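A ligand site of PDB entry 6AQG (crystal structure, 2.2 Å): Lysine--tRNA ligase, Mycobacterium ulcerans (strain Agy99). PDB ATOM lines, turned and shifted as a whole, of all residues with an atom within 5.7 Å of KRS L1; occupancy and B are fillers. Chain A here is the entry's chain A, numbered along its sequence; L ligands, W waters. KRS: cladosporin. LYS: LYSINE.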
ATOM      1  N   ARG A 263      -9.192  -1.789  19.200  1.00  0.00           N
ATOM      2  CA  ARG A 263      -7.778  -1.616  19.554  1.00  0.00           C
ATOM      3  C   ARG A 263      -7.247  -0.345  18.920  1.00  0.00           C
ATOM      4  O   ARG A 263      -7.366  -0.139  17.702  1.00  0.00           O
ATOM      5  CB  ARG A 263      -6.962  -2.855  19.164  1.00  0.00           C
ATOM      6  CG  ARG A 263      -7.624  -4.165  19.686  1.00  0.00           C
ATOM      7  CD  ARG A 263      -6.714  -5.387  19.700  1.00  0.00           C
ATOM      8  NE  ARG A 263      -7.418  -6.527  20.293  1.00  0.00           N
ATOM      9  CZ  ARG A 263      -6.975  -7.775  20.259  1.00  0.00           C
ATOM     10  NH1 ARG A 263      -5.818  -8.064  19.670  1.00  0.00           N
ATOM     11  NH2 ARG A 263      -7.693  -8.758  20.819  1.00  0.00           N
ATOM     12  N   GLU A 265      -4.893   1.303  17.577  1.00  0.00           N
ATOM     13  CA  GLU A 265      -3.595   1.100  16.938  1.00  0.00           C
ATOM     14  C   GLU A 265      -3.731   1.450  15.458  1.00  0.00           C
ATOM     15  O   GLU A 265      -4.721   2.056  15.021  1.00  0.00           O
ATOM     16  CB  GLU A 265      -3.089  -0.337  17.128  1.00  0.00           C
ATOM     17  CG  GLU A 265      -3.019  -0.836  18.580  1.00  0.00           C
ATOM     18  CD  GLU A 265      -1.797  -0.327  19.370  1.00  0.00           C
ATOM     19  OE1 GLU A 265      -1.105   0.600  18.894  1.00  0.00           O
ATOM     20  OE2 GLU A 265      -1.523  -0.864  20.476  1.00  0.00           O
ATOM     21  N   GLY A 266      -2.760   1.030  14.664  1.00  0.00           N
ATOM     22  CA  GLY A 266      -2.700   1.390  13.276  1.00  0.00           C
ATOM     23  C   GLY A 266      -3.644   0.571  12.399  1.00  0.00           C
ATOM     24  O   GLY A 266      -4.245  -0.435  12.801  1.00  0.00           O
ATOM     25  N   THR A 270      -4.464  -5.952   7.113  1.00  0.00           N
ATOM     26  CA  THR A 270      -4.880  -7.004   8.025  1.00  0.00           C
ATOM     27  C   THR A 270      -5.321  -6.473   9.390  1.00  0.00           C
ATOM     28  O   THR A 270      -5.670  -7.280  10.279  1.00  0.00           O
ATOM     29  CB  THR A 270      -3.752  -8.048   8.213  1.00  0.00           C
ATOM     30  OG1 THR A 270      -2.554  -7.402   8.660  1.00  0.00           O
ATOM     31  CG2 THR A 270      -3.451  -8.780   6.857  1.00  0.00           C
ATOM     32  N   HIS A 271      -5.348  -5.153   9.588  1.00  0.00           N
ATOM     33  CA  HIS A 271      -5.657  -4.518  10.871  1.00  0.00           C
ATOM     34  C   HIS A 271      -6.649  -3.371  10.675  1.00  0.00           C
ATOM     35  O   HIS A 271      -6.381  -2.429   9.919  1.00  0.00           O
ATOM     36  CB  HIS A 271      -4.409  -3.936  11.541  1.00  0.00           C
ATOM     37  CG  HIS A 271      -3.381  -4.944  11.922  1.00  0.00           C
ATOM     38  ND1 HIS A 271      -2.440  -5.411  11.032  1.00  0.00           N
ATOM     39  CD2 HIS A 271      -3.123  -5.561  13.099  1.00  0.00           C
ATOM     40  CE1 HIS A 271      -1.652  -6.289  11.638  1.00  0.00           C
ATOM     41  NE2 HIS A 271      -2.047  -6.395  12.896  1.00  0.00           N
ATOM     42  N   SER A 272      -7.739  -3.406  11.422  1.00  0.00           N
ATOM     43  CA  SER A 272      -8.676  -2.304  11.509  1.00  0.00           C
ATOM     44  C   SER A 272      -8.923  -2.035  12.993  1.00  0.00           C
ATOM     45  O   SER A 272      -9.215  -2.977  13.745  1.00  0.00           O
ATOM     46  CB  SER A 272      -9.956  -2.696  10.741  1.00  0.00           C
ATOM     47  OG  SER A 272     -11.068  -1.947  11.128  1.00  0.00           O
ATOM     48  N   PRO A 273      -8.785  -0.793  13.477  1.00  0.00           N
ATOM     49  CA  PRO A 273      -8.969  -0.540  14.920  1.00  0.00           C
ATOM     50  C   PRO A 273     -10.268  -1.066  15.504  1.00  0.00           C
ATOM     51  O   PRO A 273     -10.272  -1.511  16.661  1.00  0.00           O
ATOM     52  CB  PRO A 273      -8.890   0.988  15.004  1.00  0.00           C
ATOM     53  CG  PRO A 273      -7.960   1.343  13.874  1.00  0.00           C
ATOM     54  CD  PRO A 273      -8.383   0.425  12.753  1.00  0.00           C
ATOM     55  N   GLU A 274     -11.350  -1.079  14.750  1.00  0.00           N
ATOM     56  CA  GLU A 274     -12.585  -1.752  15.139  1.00  0.00           C
ATOM     57  C   GLU A 274     -12.721  -3.016  14.304  1.00  0.00           C
ATOM     58  O   GLU A 274     -12.731  -2.934  13.073  1.00  0.00           O
ATOM     59  CB  GLU A 274     -13.778  -0.826  14.915  1.00  0.00           C
ATOM     60  CG  GLU A 274     -15.105  -1.521  15.142  1.00  0.00           C
ATOM     61  CD  GLU A 274     -16.302  -0.632  14.918  1.00  0.00           C
ATOM     62  OE1 GLU A 274     -16.171   0.618  14.998  1.00  0.00           O
ATOM     63  OE2 GLU A 274     -17.395  -1.190  14.661  1.00  0.00           O
ATOM     64  N   PHE A 275     -12.858  -4.183  14.939  1.00  0.00           N
ATOM     65  CA  PHE A 275     -13.016  -5.401  14.145  1.00  0.00           C
ATOM     66  C   PHE A 275     -13.821  -6.447  14.906  1.00  0.00           C
ATOM     67  O   PHE A 275     -14.037  -6.363  16.119  1.00  0.00           O
ATOM     68  CB  PHE A 275     -11.655  -5.983  13.703  1.00  0.00           C
ATOM     69  CG  PHE A 275     -10.785  -6.505  14.837  1.00  0.00           C
ATOM     70  CD1 PHE A 275      -9.968  -5.650  15.552  1.00  0.00           C
ATOM     71  CD2 PHE A 275     -10.753  -7.861  15.137  1.00  0.00           C
ATOM     72  CE1 PHE A 275      -9.148  -6.122  16.587  1.00  0.00           C
ATOM     73  CE2 PHE A 275      -9.921  -8.339  16.171  1.00  0.00           C
ATOM     74  CZ  PHE A 275      -9.111  -7.468  16.879  1.00  0.00           C
ATOM     75  N   MET A 277     -14.483 -10.309  16.228  1.00  0.00           N
ATOM     76  CA  MET A 277     -13.698 -11.447  16.665  1.00  0.00           C
ATOM     77  C   MET A 277     -14.625 -12.466  17.294  1.00  0.00           C
ATOM     78  O   MET A 277     -15.711 -12.140  17.793  1.00  0.00           O
ATOM     79  CB  MET A 277     -12.588 -11.060  17.655  1.00  0.00           C
ATOM     80  CG  MET A 277     -13.094 -10.463  18.941  1.00  0.00           C
ATOM     81  SD  MET A 277     -13.685 -11.674  20.138  1.00  0.00           S
ATOM     82  CE  MET A 277     -15.286 -11.010  20.675  1.00  0.00           C
ATOM     83  N   LEU A 278     -14.184 -13.719  17.277  1.00  0.00           N
ATOM     84  CA  LEU A 278     -14.801 -14.815  18.007  1.00  0.00           C
ATOM     85  C   LEU A 278     -13.875 -15.235  19.154  1.00  0.00           C
ATOM     86  O   LEU A 278     -12.666 -15.360  18.965  1.00  0.00           O
ATOM     87  CB  LEU A 278     -15.016 -16.008  17.069  1.00  0.00           C
ATOM     88  CG  LEU A 278     -15.391 -17.335  17.740  1.00  0.00           C
ATOM     89  CD1 LEU A 278     -16.820 -17.289  18.244  1.00  0.00           C
ATOM     90  CD2 LEU A 278     -15.206 -18.481  16.750  1.00  0.00           C
ATOM     91  N   GLU A 279     -14.444 -15.447  20.349  1.00  0.00           N
ATOM     92  CA  GLU A 279     -13.717 -16.124  21.414  1.00  0.00           C
ATOM     93  C   GLU A 279     -14.588 -17.255  21.955  1.00  0.00           C
ATOM     94  O   GLU A 279     -15.786 -17.064  22.146  1.00  0.00           O
ATOM     95  CB  GLU A 279     -13.315 -15.187  22.569  1.00  0.00           C
ATOM     96  CG  GLU A 279     -12.070 -14.312  22.296  1.00  0.00           C
ATOM     97  CD  GLU A 279     -11.483 -13.685  23.579  1.00  0.00           C
ATOM     98  OE1 GLU A 279     -11.767 -14.225  24.671  1.00  0.00           O
ATOM     99  OE2 GLU A 279     -10.721 -12.695  23.499  1.00  0.00           O
ATOM    100  N   GLU A 423      -2.160 -14.508  10.218  1.00  0.00           N
ATOM    101  CA  GLU A 423      -2.393 -14.979  11.585  1.00  0.00           C
ATOM    102  C   GLU A 423      -3.894 -14.957  11.856  1.00  0.00           C
ATOM    103  O   GLU A 423      -4.492 -13.884  11.990  1.00  0.00           O
ATOM    104  CB  GLU A 423      -1.620 -14.116  12.589  1.00  0.00           C
ATOM    105  CG  GLU A 423      -2.030 -14.403  14.058  1.00  0.00           C
ATOM    106  CD  GLU A 423      -1.392 -13.434  15.085  1.00  0.00           C
ATOM    107  OE1 GLU A 423      -0.503 -12.614  14.726  1.00  0.00           O
ATOM    108  OE2 GLU A 423      -1.784 -13.512  16.273  1.00  0.00           O
ATOM    109  N   LEU A 424      -4.504 -16.127  11.941  1.00  0.00           N
ATOM    110  CA  LEU A 424      -5.968 -16.247  11.925  1.00  0.00           C
ATOM    111  C   LEU A 424      -6.573 -16.499  13.298  1.00  0.00           C
ATOM    112  O   LEU A 424      -7.609 -15.917  13.636  1.00  0.00           O
ATOM    113  CB  LEU A 424      -6.388 -17.370  10.973  1.00  0.00           C
ATOM    114  CG  LEU A 424      -7.886 -17.679  10.866  1.00  0.00           C
ATOM    115  CD1 LEU A 424      -8.709 -16.398  10.516  1.00  0.00           C
ATOM    116  CD2 LEU A 424      -8.130 -18.781   9.818  1.00  0.00           C
ATOM    117  N   ALA A 425      -5.960 -17.348  14.105  1.00  0.00           N
ATOM    118  CA  ALA A 425      -6.582 -17.785  15.354  1.00  0.00           C
ATOM    119  C   ALA A 425      -5.493 -18.227  16.324  1.00  0.00           C
ATOM    120  O   ALA A 425      -4.336 -18.448  15.955  1.00  0.00           O
ATOM    121  CB  ALA A 425      -7.587 -18.914  15.117  1.00  0.00           C
ATOM    122  N   THR A 426      -5.892 -18.371  17.582  1.00  0.00           N
ATOM    123  CA  THR A 426      -4.973 -18.764  18.639  1.00  0.00           C
ATOM    124  C   THR A 426      -5.782 -19.556  19.664  1.00  0.00           C
ATOM    125  O   THR A 426      -6.986 -19.384  19.770  1.00  0.00           O
ATOM    126  CB  THR A 426      -4.283 -17.524  19.256  1.00  0.00           C
ATOM    127  OG1 THR A 426      -3.236 -17.946  20.130  1.00  0.00           O
ATOM    128  CG2 THR A 426      -5.280 -16.657  20.036  1.00  0.00           C
ATOM    129  N   GLY A 477      -9.335 -17.677  20.167  1.00  0.00           N
ATOM    130  CA  GLY A 477      -9.714 -16.401  19.592  1.00  0.00           C
ATOM    131  C   GLY A 477      -9.492 -16.460  18.096  1.00  0.00           C
ATOM    132  O   GLY A 477      -8.540 -17.067  17.632  1.00  0.00           O
ATOM    133  N   MET A 478     -10.395 -15.827  17.355  1.00  0.00           N
ATOM    134  CA  MET A 478     -10.277 -15.815  15.905  1.00  0.00           C
ATOM    135  C   MET A 478     -10.787 -14.487  15.362  1.00  0.00           C
ATOM    136  O   MET A 478     -11.876 -14.052  15.741  1.00  0.00           O
ATOM    137  CB  MET A 478     -11.032 -16.995  15.275  1.00  0.00           C
ATOM    138  CG  MET A 478     -10.895 -16.997  13.726  1.00  0.00           C
ATOM    139  SD  MET A 478     -11.443 -18.542  12.960  1.00  0.00           S
ATOM    140  CE  MET A 478     -13.171 -18.454  13.305  1.00  0.00           C
ATOM    141  N   GLY A 479     -10.006 -13.865  14.483  1.00  0.00           N
ATOM    142  CA  GLY A 479     -10.463 -12.677  13.794  1.00  0.00           C
ATOM    143  C   GLY A 479     -11.452 -13.040  12.715  1.00  0.00           C
ATOM    144  O   GLY A 479     -11.122 -13.803  11.796  1.00  0.00           O
ATOM    145  N   ASP A 481     -13.072 -10.985  10.485  1.00  0.00           N
ATOM    146  CA  ASP A 481     -12.703 -10.374   9.212  1.00  0.00           C
ATOM    147  C   ASP A 481     -11.514 -11.108   8.584  1.00  0.00           C
ATOM    148  O   ASP A 481     -11.483 -11.341   7.378  1.00  0.00           O
ATOM    149  CB  ASP A 481     -12.380  -8.881   9.397  1.00  0.00           C
ATOM    150  CG  ASP A 481     -13.216  -8.239  10.509  1.00  0.00           C
ATOM    151  OD1 ASP A 481     -14.344  -7.756  10.245  1.00  0.00           O
ATOM    152  OD2 ASP A 481     -12.768  -8.277  11.675  1.00  0.00           O
ATOM    153  N   ARG A 482     -10.553 -11.506   9.414  1.00  0.00           N
ATOM    154  CA  ARG A 482      -9.432 -12.290   8.921  1.00  0.00           C
ATOM    155  C   ARG A 482      -9.885 -13.634   8.390  1.00  0.00           C
ATOM    156  O   ARG A 482      -9.354 -14.122   7.387  1.00  0.00           O
ATOM    157  CB  ARG A 482      -8.387 -12.467  10.014  1.00  0.00           C
ATOM    158  CG  ARG A 482      -7.607 -11.200  10.200  1.00  0.00           C
ATOM    159  CD  ARG A 482      -6.408 -11.425  11.023  1.00  0.00           C
ATOM    160  NE  ARG A 482      -5.641 -10.206  11.146  1.00  0.00           N
ATOM    161  CZ  ARG A 482      -4.519 -10.112  11.831  1.00  0.00           C
ATOM    162  NH1 ARG A 482      -4.042 -11.178  12.431  1.00  0.00           N
ATOM    163  NH2 ARG A 482      -3.896  -8.948  11.921  1.00  0.00           N
ATOM    164  N   ILE A 492      -8.923  -6.525   4.679  1.00  0.00           N
ATOM    165  CA  ILE A 492      -9.890  -6.378   5.774  1.00  0.00           C
ATOM    166  C   ILE A 492     -10.939  -5.323   5.434  1.00  0.00           C
ATOM    167  O   ILE A 492     -12.124  -5.495   5.755  1.00  0.00           O
ATOM    168  CB  ILE A 492      -9.140  -6.080   7.091  1.00  0.00           C
ATOM    169  CG1 ILE A 492     -10.070  -6.335   8.282  1.00  0.00           C
ATOM    170  CG2 ILE A 492      -8.646  -4.613   7.137  1.00  0.00           C
ATOM    171  CD1 ILE A 492      -9.345  -6.370   9.624  1.00  0.00           C
HETATM  172  O4  KRS L   1      -8.003  -8.658  12.657  1.00  0.00           O
HETATM  173  C8  KRS L   1      -7.300  -8.623  13.636  1.00  0.00           C
HETATM  174  C9  KRS L   1      -6.759  -7.394  14.270  1.00  0.00           C
HETATM  175  C5  KRS L   1      -5.831  -7.485  15.303  1.00  0.00           C
HETATM  176  C4  KRS L   1      -5.316  -6.375  15.910  1.00  0.00           C
HETATM  177  C3  KRS L   1      -5.721  -5.118  15.496  1.00  0.00           C
HETATM  178  O2  KRS L   1      -5.218  -4.001  16.105  1.00  0.00           O
HETATM  179  C2  KRS L   1      -6.654  -4.992  14.467  1.00  0.00           C
HETATM  180  C1  KRS L   1      -7.179  -6.117  13.836  1.00  0.00           C
HETATM  181  O1  KRS L   1      -8.080  -6.021  12.814  1.00  0.00           O
HETATM  182  O3  KRS L   1      -7.010  -9.830  14.264  1.00  0.00           O
HETATM  183  C7  KRS L   1      -6.348  -9.977  15.554  1.00  0.00           C
HETATM  184  C6  KRS L   1      -5.347  -8.841  15.787  1.00  0.00           C
HETATM  185  C10 KRS L   1      -5.678 -11.346  15.733  1.00  0.00           C
HETATM  186  C11 KRS L   1      -6.652 -12.505  15.479  1.00  0.00           C
HETATM  187  O5  KRS L   1      -7.782 -12.148  16.340  1.00  0.00           O
HETATM  188  C12 KRS L   1      -7.760 -12.406  17.768  1.00  0.00           C
HETATM  189  C16 KRS L   1      -9.159 -12.150  18.387  1.00  0.00           C
HETATM  190  C13 KRS L   1      -7.203 -13.820  18.085  1.00  0.00           C
HETATM  191  C14 KRS L   1      -5.937 -14.169  17.290  1.00  0.00           C
HETATM  192  C15 KRS L   1      -6.105 -13.921  15.776  1.00  0.00           C
HETATM  193  N   LYS L   2      -7.923 -12.654  24.014  1.00  0.00           N
HETATM  194  CA  LYS L   2      -7.170 -13.303  22.940  1.00  0.00           C
HETATM  195  C   LYS L   2      -6.674 -12.244  21.942  1.00  0.00           C
HETATM  196  O   LYS L   2      -7.276 -11.144  21.859  1.00  0.00           O
HETATM  197  CB  LYS L   2      -8.033 -14.362  22.237  1.00  0.00           C
HETATM  198  CG  LYS L   2      -8.332 -15.556  23.143  1.00  0.00           C
HETATM  199  CD  LYS L   2      -7.010 -16.120  23.659  1.00  0.00           C
HETATM  200  CE  LYS L   2      -7.283 -17.496  24.308  1.00  0.00           C
HETATM  201  NZ  LYS L   2      -7.822 -17.339  25.653  1.00  0.00           N
HETATM  202  OXT LYS L   2      -5.678 -12.459  21.206  1.00  0.00           O
HETATM  203  O   HOH W   1      -3.285  -3.925  17.910  1.00  0.00           O
HETATM  204  O   HOH W   2     -10.340  -9.866  12.061  1.00  0.00           O
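OG of Ser 272 is in hydrogen-bond range of O of Glu 274 (2.7 Å). NH2 of Arg 482 is in hydrogen-bond range of O of Thr 270 (2.9 Å). The backbone carbonyl oxygen (O) of Glu 423 sits at hydrogen-bond distance from the guanidinium group (NH1) of Arg 482, at 2.8 Å. O of Leu 424 is in hydrogen-bond range of N of Gly 479, 3.3 Å away. The side-chain hydroxyl of Thr 270 is in hydrogen-bond range of a ring nitrogen (ND1) of His 271 (3.1 Å). The backbone carbonyl oxygen of Thr 426 lies within hydrogen-bond range of the backbone NH of Gly 477, at 2.9 Å. N of Arg 263 sits at hydrogen-bond distance from O of Pro 273 (2.8 Å). The backbone carbonyl oxygen (O) of Met 478 sits at hydrogen-bond distance from the backbone NH (N) of Leu 278 (2.8 Å).
O1 of KRS L1 sits at hydrogen-bond distance from N of Ser 272. O of Ser 272 lies close to O1 of KRS L1 (3.4 Å). An oxygen (O4) of KRS L1 lies within hydrogen-bond range of the guanidinium group (NE) of Arg 482 (3.2 Å). N of Gly 479 sits at hydrogen-bond distance from O5 of KRS L1, at 3.4 Å. The guanidinium group of Arg 263 lies within salt-bridge range of an oxygen (O) of LYS L2 (2.6 Å). OE2 of Glu 279 lies within salt-bridge range of N of LYS L2, 2.8 Å away.
Arg 263 touches KRS L1. Thr 270 touches KRS L1 (O to O4, 3.6 Å). CA of His 271 touches O1 of KRS L1 (3.5 Å). Phe 275 touches KRS L1. Met 277 touches KRS L1. Leu 424 touches KRS L1 (O to C15, 3.3 Å). N of Ala 425 touches C15 of KRS L1 (3.8 Å). CG2 of Thr 426 touches C14 of KRS L1 (3.8 Å). Gly 477 touches KRS L1 (C to C13, 3.5 Å). N of Met 478 touches C13 of KRS L1, 3.8 Å away. Ile 492 touches KRS L1 (CD1 to O1, 3.4 Å). Hydrophobic or aromatic side chains within 4 Å of KRS L1: His 271, Phe 275, Met 277 and Ile 492. Within 4 Å of KRS L1: Arg 263, Thr 270, His 271, Ser 272, Phe 275, Met 277, Leu 424, Ala 425, Thr 426, Gly 477, Met 478, Gly 479, Arg 482 and Ile 492.
Water W2 lies within hydrogen-bond range of an oxygen (O4) of KRS L1 (2.7 Å), the side-chain carboxylate of Asp 481 (2.9 Å) and the backbone NH of Arg 482 (3.1 Å).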
